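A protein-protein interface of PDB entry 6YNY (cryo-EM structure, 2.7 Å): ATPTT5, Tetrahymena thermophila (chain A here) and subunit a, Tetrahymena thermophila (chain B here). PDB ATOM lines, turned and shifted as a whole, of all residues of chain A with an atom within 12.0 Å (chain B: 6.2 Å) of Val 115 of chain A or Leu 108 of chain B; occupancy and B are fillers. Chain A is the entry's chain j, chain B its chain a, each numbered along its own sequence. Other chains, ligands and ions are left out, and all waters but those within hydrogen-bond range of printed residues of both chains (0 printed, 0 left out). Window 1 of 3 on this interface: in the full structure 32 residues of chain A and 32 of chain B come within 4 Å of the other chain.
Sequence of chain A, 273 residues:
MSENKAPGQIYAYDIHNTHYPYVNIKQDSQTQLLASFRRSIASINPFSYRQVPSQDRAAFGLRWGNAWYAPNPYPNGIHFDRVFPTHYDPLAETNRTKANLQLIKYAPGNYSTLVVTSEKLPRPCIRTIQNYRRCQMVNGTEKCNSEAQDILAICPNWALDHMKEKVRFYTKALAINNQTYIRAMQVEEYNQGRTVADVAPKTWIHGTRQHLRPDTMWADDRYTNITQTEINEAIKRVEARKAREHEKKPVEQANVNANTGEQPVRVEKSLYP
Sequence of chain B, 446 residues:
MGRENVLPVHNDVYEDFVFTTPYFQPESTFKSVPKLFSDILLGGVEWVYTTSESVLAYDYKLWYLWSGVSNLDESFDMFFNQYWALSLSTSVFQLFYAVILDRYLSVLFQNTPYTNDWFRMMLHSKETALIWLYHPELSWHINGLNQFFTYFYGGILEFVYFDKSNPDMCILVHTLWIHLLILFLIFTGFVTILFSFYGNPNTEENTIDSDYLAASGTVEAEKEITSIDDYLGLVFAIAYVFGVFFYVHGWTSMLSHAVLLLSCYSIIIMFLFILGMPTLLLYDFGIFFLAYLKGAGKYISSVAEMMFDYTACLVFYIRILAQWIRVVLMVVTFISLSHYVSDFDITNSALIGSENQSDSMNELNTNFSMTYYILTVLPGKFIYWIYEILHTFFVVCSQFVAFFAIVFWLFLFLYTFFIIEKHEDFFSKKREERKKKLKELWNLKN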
ATOM      1  N   PRO A 108      44.424  32.868  -0.339  1.00  0.00           N
ATOM      2  CA  PRO A 108      44.292  31.548  -0.950  1.00  0.00           C
ATOM      3  C   PRO A 108      43.139  31.500  -1.939  1.00  0.00           C
ATOM      4  O   PRO A 108      42.209  32.307  -1.902  1.00  0.00           O
ATOM      5  CB  PRO A 108      44.032  30.635   0.248  1.00  0.00           C
ATOM      6  CG  PRO A 108      43.372  31.506   1.230  1.00  0.00           C
ATOM      7  CD  PRO A 108      43.970  32.867   1.060  1.00  0.00           C
ATOM      8  N   GLY A 109      43.218  30.523  -2.833  1.00  0.00           N
ATOM      9  CA  GLY A 109      42.188  30.324  -3.827  1.00  0.00           C
ATOM     10  C   GLY A 109      42.229  31.336  -4.950  1.00  0.00           C
ATOM     11  O   GLY A 109      41.303  32.137  -5.107  1.00  0.00           O
ATOM     12  N   TYR A 111      41.698  30.747  -7.954  1.00  0.00           N
ATOM     13  CA  TYR A 111      40.504  30.417  -8.722  1.00  0.00           C
ATOM     14  C   TYR A 111      39.584  29.636  -7.797  1.00  0.00           C
ATOM     15  O   TYR A 111      39.599  28.405  -7.776  1.00  0.00           O
ATOM     16  CB  TYR A 111      40.865  29.632  -9.971  1.00  0.00           C
ATOM     17  CG  TYR A 111      42.009  30.243 -10.734  1.00  0.00           C
ATOM     18  CD1 TYR A 111      41.804  31.302 -11.602  1.00  0.00           C
ATOM     19  CD2 TYR A 111      43.298  29.767 -10.581  1.00  0.00           C
ATOM     20  CE1 TYR A 111      42.846  31.864 -12.292  1.00  0.00           C
ATOM     21  CE2 TYR A 111      44.344  30.323 -11.270  1.00  0.00           C
ATOM     22  CZ  TYR A 111      44.114  31.371 -12.124  1.00  0.00           C
ATOM     23  OH  TYR A 111      45.155  31.933 -12.815  1.00  0.00           O
ATOM     24  N   SER A 112      38.777  30.363  -7.031  1.00  0.00           N
ATOM     25  CA  SER A 112      37.895  29.748  -6.057  1.00  0.00           C
ATOM     26  C   SER A 112      36.623  30.566  -5.949  1.00  0.00           C
ATOM     27  O   SER A 112      36.610  31.766  -6.231  1.00  0.00           O
ATOM     28  CB  SER A 112      38.563  29.629  -4.683  1.00  0.00           C
ATOM     29  OG  SER A 112      38.899  30.899  -4.164  1.00  0.00           O
ATOM     30  N   THR A 113      35.553  29.897  -5.543  1.00  0.00           N
ATOM     31  CA  THR A 113      34.262  30.522  -5.325  1.00  0.00           C
ATOM     32  C   THR A 113      33.737  30.126  -3.954  1.00  0.00           C
ATOM     33  O   THR A 113      34.238  29.203  -3.310  1.00  0.00           O
ATOM     34  CB  THR A 113      33.251  30.124  -6.406  1.00  0.00           C
ATOM     35  OG1 THR A 113      33.024  28.713  -6.360  1.00  0.00           O
ATOM     36  CG2 THR A 113      33.762  30.504  -7.776  1.00  0.00           C
ATOM     37  N   LEU A 114      32.711  30.844  -3.517  1.00  0.00           N
ATOM     38  CA  LEU A 114      32.092  30.621  -2.219  1.00  0.00           C
ATOM     39  C   LEU A 114      30.892  29.698  -2.388  1.00  0.00           C
ATOM     40  O   LEU A 114      29.961  30.013  -3.136  1.00  0.00           O
ATOM     41  CB  LEU A 114      31.677  31.949  -1.596  1.00  0.00           C
ATOM     42  CG  LEU A 114      30.969  31.894  -0.247  1.00  0.00           C
ATOM     43  CD1 LEU A 114      31.839  31.228   0.786  1.00  0.00           C
ATOM     44  CD2 LEU A 114      30.608  33.289   0.184  1.00  0.00           C
ATOM     45  N   VAL A 115      30.921  28.560  -1.701  1.00  0.00           N
ATOM     46  CA  VAL A 115      29.843  27.590  -1.723  1.00  0.00           C
ATOM     47  C   VAL A 115      29.492  27.214  -0.290  1.00  0.00           C
ATOM     48  O   VAL A 115      30.129  27.647   0.667  1.00  0.00           O
ATOM     49  CB  VAL A 115      30.197  26.327  -2.533  1.00  0.00           C
ATOM     50  CG1 VAL A 115      30.567  26.680  -3.950  1.00  0.00           C
ATOM     51  CG2 VAL A 115      31.302  25.553  -1.849  1.00  0.00           C
ATOM     52  N   VAL A 116      28.459  26.392  -0.161  1.00  0.00           N
ATOM     53  CA  VAL A 116      28.037  25.828   1.110  1.00  0.00           C
ATOM     54  C   VAL A 116      28.121  24.315   0.990  1.00  0.00           C
ATOM     55  O   VAL A 116      27.646  23.738   0.005  1.00  0.00           O
ATOM     56  CB  VAL A 116      26.616  26.281   1.486  1.00  0.00           C
ATOM     57  CG1 VAL A 116      25.601  25.626   0.599  1.00  0.00           C
ATOM     58  CG2 VAL A 116      26.329  25.976   2.922  1.00  0.00           C
ATOM     59  N   THR A 117      28.744  23.678   1.975  1.00  0.00           N
ATOM     60  CA  THR A 117      28.919  22.237   1.989  1.00  0.00           C
ATOM     61  C   THR A 117      28.364  21.680   3.292  1.00  0.00           C
ATOM     62  O   THR A 117      27.940  22.421   4.183  1.00  0.00           O
ATOM     63  CB  THR A 117      30.391  21.844   1.809  1.00  0.00           C
ATOM     64  OG1 THR A 117      30.506  20.418   1.773  1.00  0.00           O
ATOM     65  CG2 THR A 117      31.244  22.381   2.937  1.00  0.00           C
ATOM     66  N   SER A 118      28.371  20.355   3.394  1.00  0.00           N
ATOM     67  CA  SER A 118      27.816  19.662   4.545  1.00  0.00           C
ATOM     68  C   SER A 118      28.619  18.398   4.790  1.00  0.00           C
ATOM     69  O   SER A 118      28.922  17.662   3.847  1.00  0.00           O
ATOM     70  CB  SER A 118      26.341  19.321   4.318  1.00  0.00           C
ATOM     71  OG  SER A 118      25.801  18.613   5.418  1.00  0.00           O
ATOM     72  N   GLU A 119      28.972  18.160   6.049  1.00  0.00           N
ATOM     73  CA  GLU A 119      29.620  16.910   6.414  1.00  0.00           C
ATOM     74  C   GLU A 119      28.625  15.763   6.324  1.00  0.00           C
ATOM     75  O   GLU A 119      27.443  15.914   6.645  1.00  0.00           O
ATOM     76  CB  GLU A 119      30.187  16.999   7.829  1.00  0.00           C
ATOM     77  CG  GLU A 119      31.397  17.908   7.977  1.00  0.00           C
ATOM     78  CD  GLU A 119      32.666  17.299   7.407  1.00  0.00           C
ATOM     79  OE1 GLU A 119      32.570  16.321   6.636  1.00  0.00           O
ATOM     80  OE2 GLU A 119      33.763  17.796   7.741  1.00  0.00           O
ATOM     81  N   PHE A 169      18.864  26.080  12.472  1.00  0.00           N
ATOM     82  CA  PHE A 169      19.049  26.870  11.262  1.00  0.00           C
ATOM     83  C   PHE A 169      17.764  26.934  10.449  1.00  0.00           C
ATOM     84  O   PHE A 169      17.313  28.018  10.064  1.00  0.00           O
ATOM     85  CB  PHE A 169      20.177  26.295  10.412  1.00  0.00           C
ATOM     86  CG  PHE A 169      20.178  26.810   9.010  1.00  0.00           C
ATOM     87  CD1 PHE A 169      20.600  28.093   8.738  1.00  0.00           C
ATOM     88  CD2 PHE A 169      19.735  26.025   7.966  1.00  0.00           C
ATOM     89  CE1 PHE A 169      20.587  28.578   7.461  1.00  0.00           C
ATOM     90  CE2 PHE A 169      19.724  26.509   6.683  1.00  0.00           C
ATOM     91  CZ  PHE A 169      20.152  27.788   6.431  1.00  0.00           C
ATOM     92  N   ASP B  77      30.198  26.165 -19.533  1.00  0.00           N
ATOM     93  CA  ASP B  77      28.804  26.126 -19.096  1.00  0.00           C
ATOM     94  C   ASP B  77      27.932  26.565 -20.263  1.00  0.00           C
ATOM     95  O   ASP B  77      27.694  27.752 -20.482  1.00  0.00           O
ATOM     96  CB  ASP B  77      28.599  27.012 -17.876  1.00  0.00           C
ATOM     97  CG  ASP B  77      27.282  26.742 -17.176  1.00  0.00           C
ATOM     98  OD1 ASP B  77      26.306  26.375 -17.860  1.00  0.00           O
ATOM     99  OD2 ASP B  77      27.225  26.892 -15.938  1.00  0.00           O
ATOM    100  N   ARG B 103      18.279  30.786 -10.270  1.00  0.00           N
ATOM    101  CA  ARG B 103      18.127  29.526  -9.559  1.00  0.00           C
ATOM    102  C   ARG B 103      19.230  28.543  -9.919  1.00  0.00           C
ATOM    103  O   ARG B 103      19.575  27.679  -9.107  1.00  0.00           O
ATOM    104  CB  ARG B 103      16.760  28.921  -9.860  1.00  0.00           C
ATOM    105  CG  ARG B 103      15.601  29.754  -9.367  1.00  0.00           C
ATOM    106  CD  ARG B 103      15.490  29.739  -7.860  1.00  0.00           C
ATOM    107  NE  ARG B 103      15.227  28.401  -7.344  1.00  0.00           N
ATOM    108  CZ  ARG B 103      14.895  28.140  -6.085  1.00  0.00           C
ATOM    109  NH1 ARG B 103      14.778  29.126  -5.208  1.00  0.00           N
ATOM    110  NH2 ARG B 103      14.672  26.891  -5.705  1.00  0.00           N
ATOM    111  N   TYR B 104      19.790  28.659 -11.121  1.00  0.00           N
ATOM    112  CA  TYR B 104      20.928  27.834 -11.495  1.00  0.00           C
ATOM    113  C   TYR B 104      22.164  28.204 -10.689  1.00  0.00           C
ATOM    114  O   TYR B 104      22.973  27.330 -10.358  1.00  0.00           O
ATOM    115  CB  TYR B 104      21.196  27.979 -12.990  1.00  0.00           C
ATOM    116  CG  TYR B 104      22.419  27.247 -13.482  1.00  0.00           C
ATOM    117  CD1 TYR B 104      22.388  25.883 -13.703  1.00  0.00           C
ATOM    118  CD2 TYR B 104      23.600  27.923 -13.739  1.00  0.00           C
ATOM    119  CE1 TYR B 104      23.496  25.213 -14.155  1.00  0.00           C
ATOM    120  CE2 TYR B 104      24.712  27.259 -14.190  1.00  0.00           C
ATOM    121  CZ  TYR B 104      24.656  25.905 -14.398  1.00  0.00           C
ATOM    122  OH  TYR B 104      25.769  25.239 -14.850  1.00  0.00           O
ATOM    123  N   LEU B 105      22.324  29.487 -10.366  1.00  0.00           N
ATOM    124  CA  LEU B 105      23.447  29.917  -9.545  1.00  0.00           C
ATOM    125  C   LEU B 105      23.291  29.479  -8.096  1.00  0.00           C
ATOM    126  O   LEU B 105      24.292  29.258  -7.408  1.00  0.00           O
ATOM    127  CB  LEU B 105      23.595  31.432  -9.623  1.00  0.00           C
ATOM    128  CG  LEU B 105      23.950  31.998 -10.996  1.00  0.00           C
ATOM    129  CD1 LEU B 105      24.026  33.500 -10.927  1.00  0.00           C
ATOM    130  CD2 LEU B 105      25.252  31.422 -11.504  1.00  0.00           C
ATOM    131  N   SER B 106      22.056  29.351  -7.616  1.00  0.00           N
ATOM    132  CA  SER B 106      21.830  28.860  -6.266  1.00  0.00           C
ATOM    133  C   SER B 106      22.079  27.366  -6.146  1.00  0.00           C
ATOM    134  O   SER B 106      22.166  26.856  -5.024  1.00  0.00           O
ATOM    135  CB  SER B 106      20.407  29.180  -5.825  1.00  0.00           C
ATOM    136  OG  SER B 106      19.467  28.474  -6.610  1.00  0.00           O
ATOM    137  N   VAL B 107      22.184  26.661  -7.269  1.00  0.00           N
ATOM    138  CA  VAL B 107      22.512  25.242  -7.247  1.00  0.00           C
ATOM    139  C   VAL B 107      24.018  25.040  -7.180  1.00  0.00           C
ATOM    140  O   VAL B 107      24.515  24.231  -6.388  1.00  0.00           O
ATOM    141  CB  VAL B 107      21.903  24.546  -8.474  1.00  0.00           C
ATOM    142  CG1 VAL B 107      22.464  23.157  -8.617  1.00  0.00           C
ATOM    143  CG2 VAL B 107      20.398  24.508  -8.353  1.00  0.00           C
ATOM    144  N   LEU B 108      24.766  25.763  -8.015  1.00  0.00           N
ATOM    145  CA  LEU B 108      26.220  25.726  -7.925  1.00  0.00           C
ATOM    146  C   LEU B 108      26.702  26.101  -6.534  1.00  0.00           C
ATOM    147  O   LEU B 108      27.761  25.639  -6.095  1.00  0.00           O
ATOM    148  CB  LEU B 108      26.830  26.680  -8.946  1.00  0.00           C
ATOM    149  CG  LEU B 108      26.491  26.470 -10.414  1.00  0.00           C
ATOM    150  CD1 LEU B 108      27.149  27.564 -11.216  1.00  0.00           C
ATOM    151  CD2 LEU B 108      26.934  25.105 -10.889  1.00  0.00           C
ATOM    152  N   PHE B 109      25.944  26.939  -5.834  1.00  0.00           N
ATOM    153  CA  PHE B 109      26.307  27.356  -4.491  1.00  0.00           C
ATOM    154  C   PHE B 109      26.234  26.214  -3.485  1.00  0.00           C
ATOM    155  O   PHE B 109      26.834  26.316  -2.410  1.00  0.00           O
ATOM    156  CB  PHE B 109      25.398  28.515  -4.083  1.00  0.00           C
ATOM    157  CG  PHE B 109      25.383  28.801  -2.621  1.00  0.00           C
ATOM    158  CD1 PHE B 109      26.473  29.371  -2.001  1.00  0.00           C
ATOM    159  CD2 PHE B 109      24.259  28.530  -1.870  1.00  0.00           C
ATOM    160  CE1 PHE B 109      26.450  29.643  -0.652  1.00  0.00           C
ATOM    161  CE2 PHE B 109      24.230  28.798  -0.529  1.00  0.00           C
ATOM    162  CZ  PHE B 109      25.325  29.360   0.085  1.00  0.00           C
ATOM    163  N   GLN B 110      25.540  25.129  -3.814  1.00  0.00           N
ATOM    164  CA  GLN B 110      25.363  23.988  -2.919  1.00  0.00           C
ATOM    165  C   GLN B 110      26.241  22.838  -3.406  1.00  0.00           C
ATOM    166  O   GLN B 110      25.808  22.002  -4.200  1.00  0.00           O
ATOM    167  CB  GLN B 110      23.901  23.578  -2.859  1.00  0.00           C
ATOM    168  CG  GLN B 110      22.980  24.654  -2.342  1.00  0.00           C
ATOM    169  CD  GLN B 110      21.528  24.250  -2.412  1.00  0.00           C
ATOM    170  OE1 GLN B 110      21.161  23.140  -2.034  1.00  0.00           O
ATOM    171  NE2 GLN B 110      20.693  25.147  -2.912  1.00  0.00           N
ATOM    172  N   ASN B 111      27.482  22.804  -2.929  1.00  0.00           N
ATOM    173  CA  ASN B 111      28.414  21.729  -3.265  1.00  0.00           C
ATOM    174  C   ASN B 111      28.470  20.712  -2.124  1.00  0.00           C
ATOM    175  O   ASN B 111      29.460  20.584  -1.406  1.00  0.00           O
ATOM    176  CB  ASN B 111      29.789  22.302  -3.578  1.00  0.00           C
ATOM    177  CG  ASN B 111      30.680  21.313  -4.284  1.00  0.00           C
ATOM    178  OD1 ASN B 111      31.428  20.567  -3.655  1.00  0.00           O
ATOM    179  ND2 ASN B 111      30.603  21.299  -5.607  1.00  0.00           N
ATOM    180  N   HIS B 124      24.802  18.104 -11.935  1.00  0.00           N
ATOM    181  CA  HIS B 124      25.915  18.732 -11.241  1.00  0.00           C
ATOM    182  C   HIS B 124      27.267  18.376 -11.824  1.00  0.00           C
ATOM    183  O   HIS B 124      28.230  19.113 -11.588  1.00  0.00           O
ATOM    184  CB  HIS B 124      25.914  18.349  -9.758  1.00  0.00           C
ATOM    185  CG  HIS B 124      24.648  18.693  -9.046  1.00  0.00           C
ATOM    186  ND1 HIS B 124      24.374  19.966  -8.599  1.00  0.00           N
ATOM    187  CD2 HIS B 124      23.585  17.932  -8.697  1.00  0.00           C
ATOM    188  CE1 HIS B 124      23.193  19.976  -8.010  1.00  0.00           C
ATOM    189  NE2 HIS B 124      22.693  18.755  -8.055  1.00  0.00           N
ATOM    190  N   GLU B 158      27.994  24.473   5.962  1.00  0.00           N
ATOM    191  CA  GLU B 158      29.182  25.262   6.247  1.00  0.00           C
ATOM    192  C   GLU B 158      29.678  25.945   4.980  1.00  0.00           C
ATOM    193  O   GLU B 158      29.708  25.340   3.905  1.00  0.00           O
ATOM    194  CB  GLU B 158      30.290  24.381   6.826  1.00  0.00           C
ATOM    195  CG  GLU B 158      29.893  23.648   8.092  1.00  0.00           C
ATOM    196  CD  GLU B 158      30.972  22.707   8.591  1.00  0.00           C
ATOM    197  OE1 GLU B 158      31.903  22.402   7.817  1.00  0.00           O
ATOM    198  OE2 GLU B 158      30.889  22.271   9.758  1.00  0.00           O
ATOM    199  N   PHE B 159      30.069  27.207   5.119  1.00  0.00           N
ATOM    200  CA  PHE B 159      30.590  27.979   4.001  1.00  0.00           C
ATOM    201  C   PHE B 159      32.076  27.703   3.831  1.00  0.00           C
ATOM    202  O   PHE B 159      32.859  27.885   4.768  1.00  0.00           O
ATOM    203  CB  PHE B 159      30.346  29.467   4.217  1.00  0.00           C
ATOM    204  CG  PHE B 159      28.933  29.886   3.996  1.00  0.00           C
ATOM    205  CD1 PHE B 159      28.501  30.252   2.739  1.00  0.00           C
ATOM    206  CD2 PHE B 159      28.037  29.923   5.042  1.00  0.00           C
ATOM    207  CE1 PHE B 159      27.206  30.640   2.530  1.00  0.00           C
ATOM    208  CE2 PHE B 159      26.739  30.312   4.834  1.00  0.00           C
ATOM    209  CZ  PHE B 159      26.324  30.670   3.577  1.00  0.00           C
ATOM    210  N   VAL B 160      32.461  27.260   2.638  1.00  0.00           N
ATOM    211  CA  VAL B 160      33.855  27.046   2.288  1.00  0.00           C
ATOM    212  C   VAL B 160      34.097  27.643   0.911  1.00  0.00           C
ATOM    213  O   VAL B 160      33.166  27.904   0.148  1.00  0.00           O
ATOM    214  CB  VAL B 160      34.242  25.554   2.298  1.00  0.00           C
ATOM    215  CG1 VAL B 160      33.931  24.933   3.635  1.00  0.00           C
ATOM    216  CG2 VAL B 160      33.529  24.818   1.195  1.00  0.00           C
ATOM    217  N   TYR B 161      35.370  27.860   0.601  1.00  0.00           N
ATOM    218  CA  TYR B 161      35.768  28.357  -0.706  1.00  0.00           C
ATOM    219  C   TYR B 161      36.080  27.166  -1.604  1.00  0.00           C
ATOM    220  O   TYR B 161      36.928  26.333  -1.271  1.00  0.00           O
ATOM    221  CB  TYR B 161      36.963  29.299  -0.593  1.00  0.00           C
ATOM    222  CG  TYR B 161      36.667  30.565   0.175  1.00  0.00           C
ATOM    223  CD1 TYR B 161      35.738  31.477  -0.292  1.00  0.00           C
ATOM    224  CD2 TYR B 161      37.318  30.849   1.361  1.00  0.00           C
ATOM    225  CE1 TYR B 161      35.464  32.626   0.403  1.00  0.00           C
ATOM    226  CE2 TYR B 161      37.048  31.998   2.059  1.00  0.00           C
ATOM    227  CZ  TYR B 161      36.122  32.885   1.576  1.00  0.00           C
ATOM    228  OH  TYR B 161      35.851  34.036   2.274  1.00  0.00           O
ATOM    229  N   PHE B 162      35.380  27.086  -2.729  1.00  0.00           N
ATOM    230  CA  PHE B 162      35.452  25.945  -3.633  1.00  0.00           C
ATOM    231  C   PHE B 162      36.544  26.194  -4.665  1.00  0.00           C
ATOM    232  O   PHE B 162      36.416  27.081  -5.514  1.00  0.00           O
ATOM    233  CB  PHE B 162      34.093  25.731  -4.290  1.00  0.00           C
ATOM    234  CG  PHE B 162      34.037  24.572  -5.228  1.00  0.00           C
ATOM    235  CD1 PHE B 162      33.989  24.776  -6.589  1.00  0.00           C
ATOM    236  CD2 PHE B 162      34.009  23.279  -4.753  1.00  0.00           C
ATOM    237  CE1 PHE B 162      33.924  23.717  -7.457  1.00  0.00           C
ATOM    238  CE2 PHE B 162      33.944  22.216  -5.618  1.00  0.00           C
ATOM    239  CZ  PHE B 162      33.902  22.435  -6.970  1.00  0.00           C
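The backbone NH (N) of Val 116 of chain A is in hydrogen-bond range of the backbone carbonyl oxygen (O) of Phe 109 of chain B, 2.8 Å away. O of Val 116 of chain A sits at hydrogen-bond distance from N of Asn 111 of chain B, 3.1 Å away. The backbone carbonyl oxygen (O) of Asn 111 of chain B sits at hydrogen-bond distance from the side-chain hydroxyl (OG1) of Thr 117 of chain A, 3.4 Å away. The backbone NH (N) of Glu 158 of chain B sits at hydrogen-bond distance from the backbone carbonyl oxygen (O) of Thr 117 of chain A, 2.7 Å away. The backbone NH (N) of Val 115 of chain A sits at hydrogen-bond distance from the backbone carbonyl oxygen (O) of Val 160 of chain B, at 3.0 Å. N of Phe 162 of chain B lies within hydrogen-bond range of O of Thr 113 of chain A, 2.5 Å away.
Along chain B the printed residues that touch a printed residue of chain A span positions 108 to 162. Of the 12 printed residues of chain A, 6 touch a printed residue of chain B. Printed residues of chain A that touch a printed residue of chain B: Ser 112, Thr 113, Leu 114, Val 115, Val 116 and Thr 117. Hydrophobic or aromatic side chains of chain A within 4 Å of the printed part of chain B: Leu 114, Val 115 and Val 116. Among the printed residues, no Asp or Glu carboxylate lies within 4 Å of a Lys or Arg side-chain nitrogen of the other chain.
The side-chain amide nitrogen of Gln 110 of chain B lies within hydrogen-bond range of the backbone carbonyl oxygen of Ser 106 of chain B (3.1 Å). The backbone carbonyl oxygen (O) of Gly 109 of chain A lies within hydrogen-bond range of the side-chain hydroxyl (OG) of Ser 112 of chain A.
Among the printed residues, merely in contact across the chains: Ser 112 of chain A with Phe 162 of chain B, Thr 113 of chain A with Tyr 161 of chain B, Val 116 of chain A with Glu 158 of chain B, Val 115 of chain A with Phe 109 of chain B, Val 115 of chain A with Phe 159 of chain B, Leu 114 of chain A with Val 160 of chain B, Val 115 of chain A with Phe 162 of chain B, Val 115 of chain A with Leu 108 of chain B, Val 116 of chain A with Gln 110 of chain B, Leu 114 of chain A with Phe 109 of chain B, Thr 117 of chain A with Val 160 of chain B, Thr 113 of chain A with Val 160 of chain B, Leu 114 of chain A with Tyr 161 of chain B, Val 115 of chain A with Asn 111 of chain B, Leu 114 of chain A with Phe 159 of chain B and Val 115 of chain A with Glu 158 of chain B.
Leu 108 of chain B touches just one residue of chain A: Val 115 (3.7 Å). No residue of chain A comes within 4 Å of Tyr 104 of chain B. No residue of chain A comes within 4 Å of Leu 105 of chain B. No residue of chain A comes within 4 Å of Ser 106 of chain B. No residue of chain A comes within 4 Å of Val 107 of chain B. Phe 109 of chain B touches three residues of chain A. No residue of chain A comes within 4 Å of His 124 of chain B. Phe 162 of chain B touches three residues of chain A. Printed residues of chain B within 4 Å of Thr 113 of chain A: Val 160 (3.8 Å), Tyr 161 (3.1 Å) and Phe 162 (2.5 Å). Printed residues of chain B within 4 Å of Ser 112 of chain A: Phe 162.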
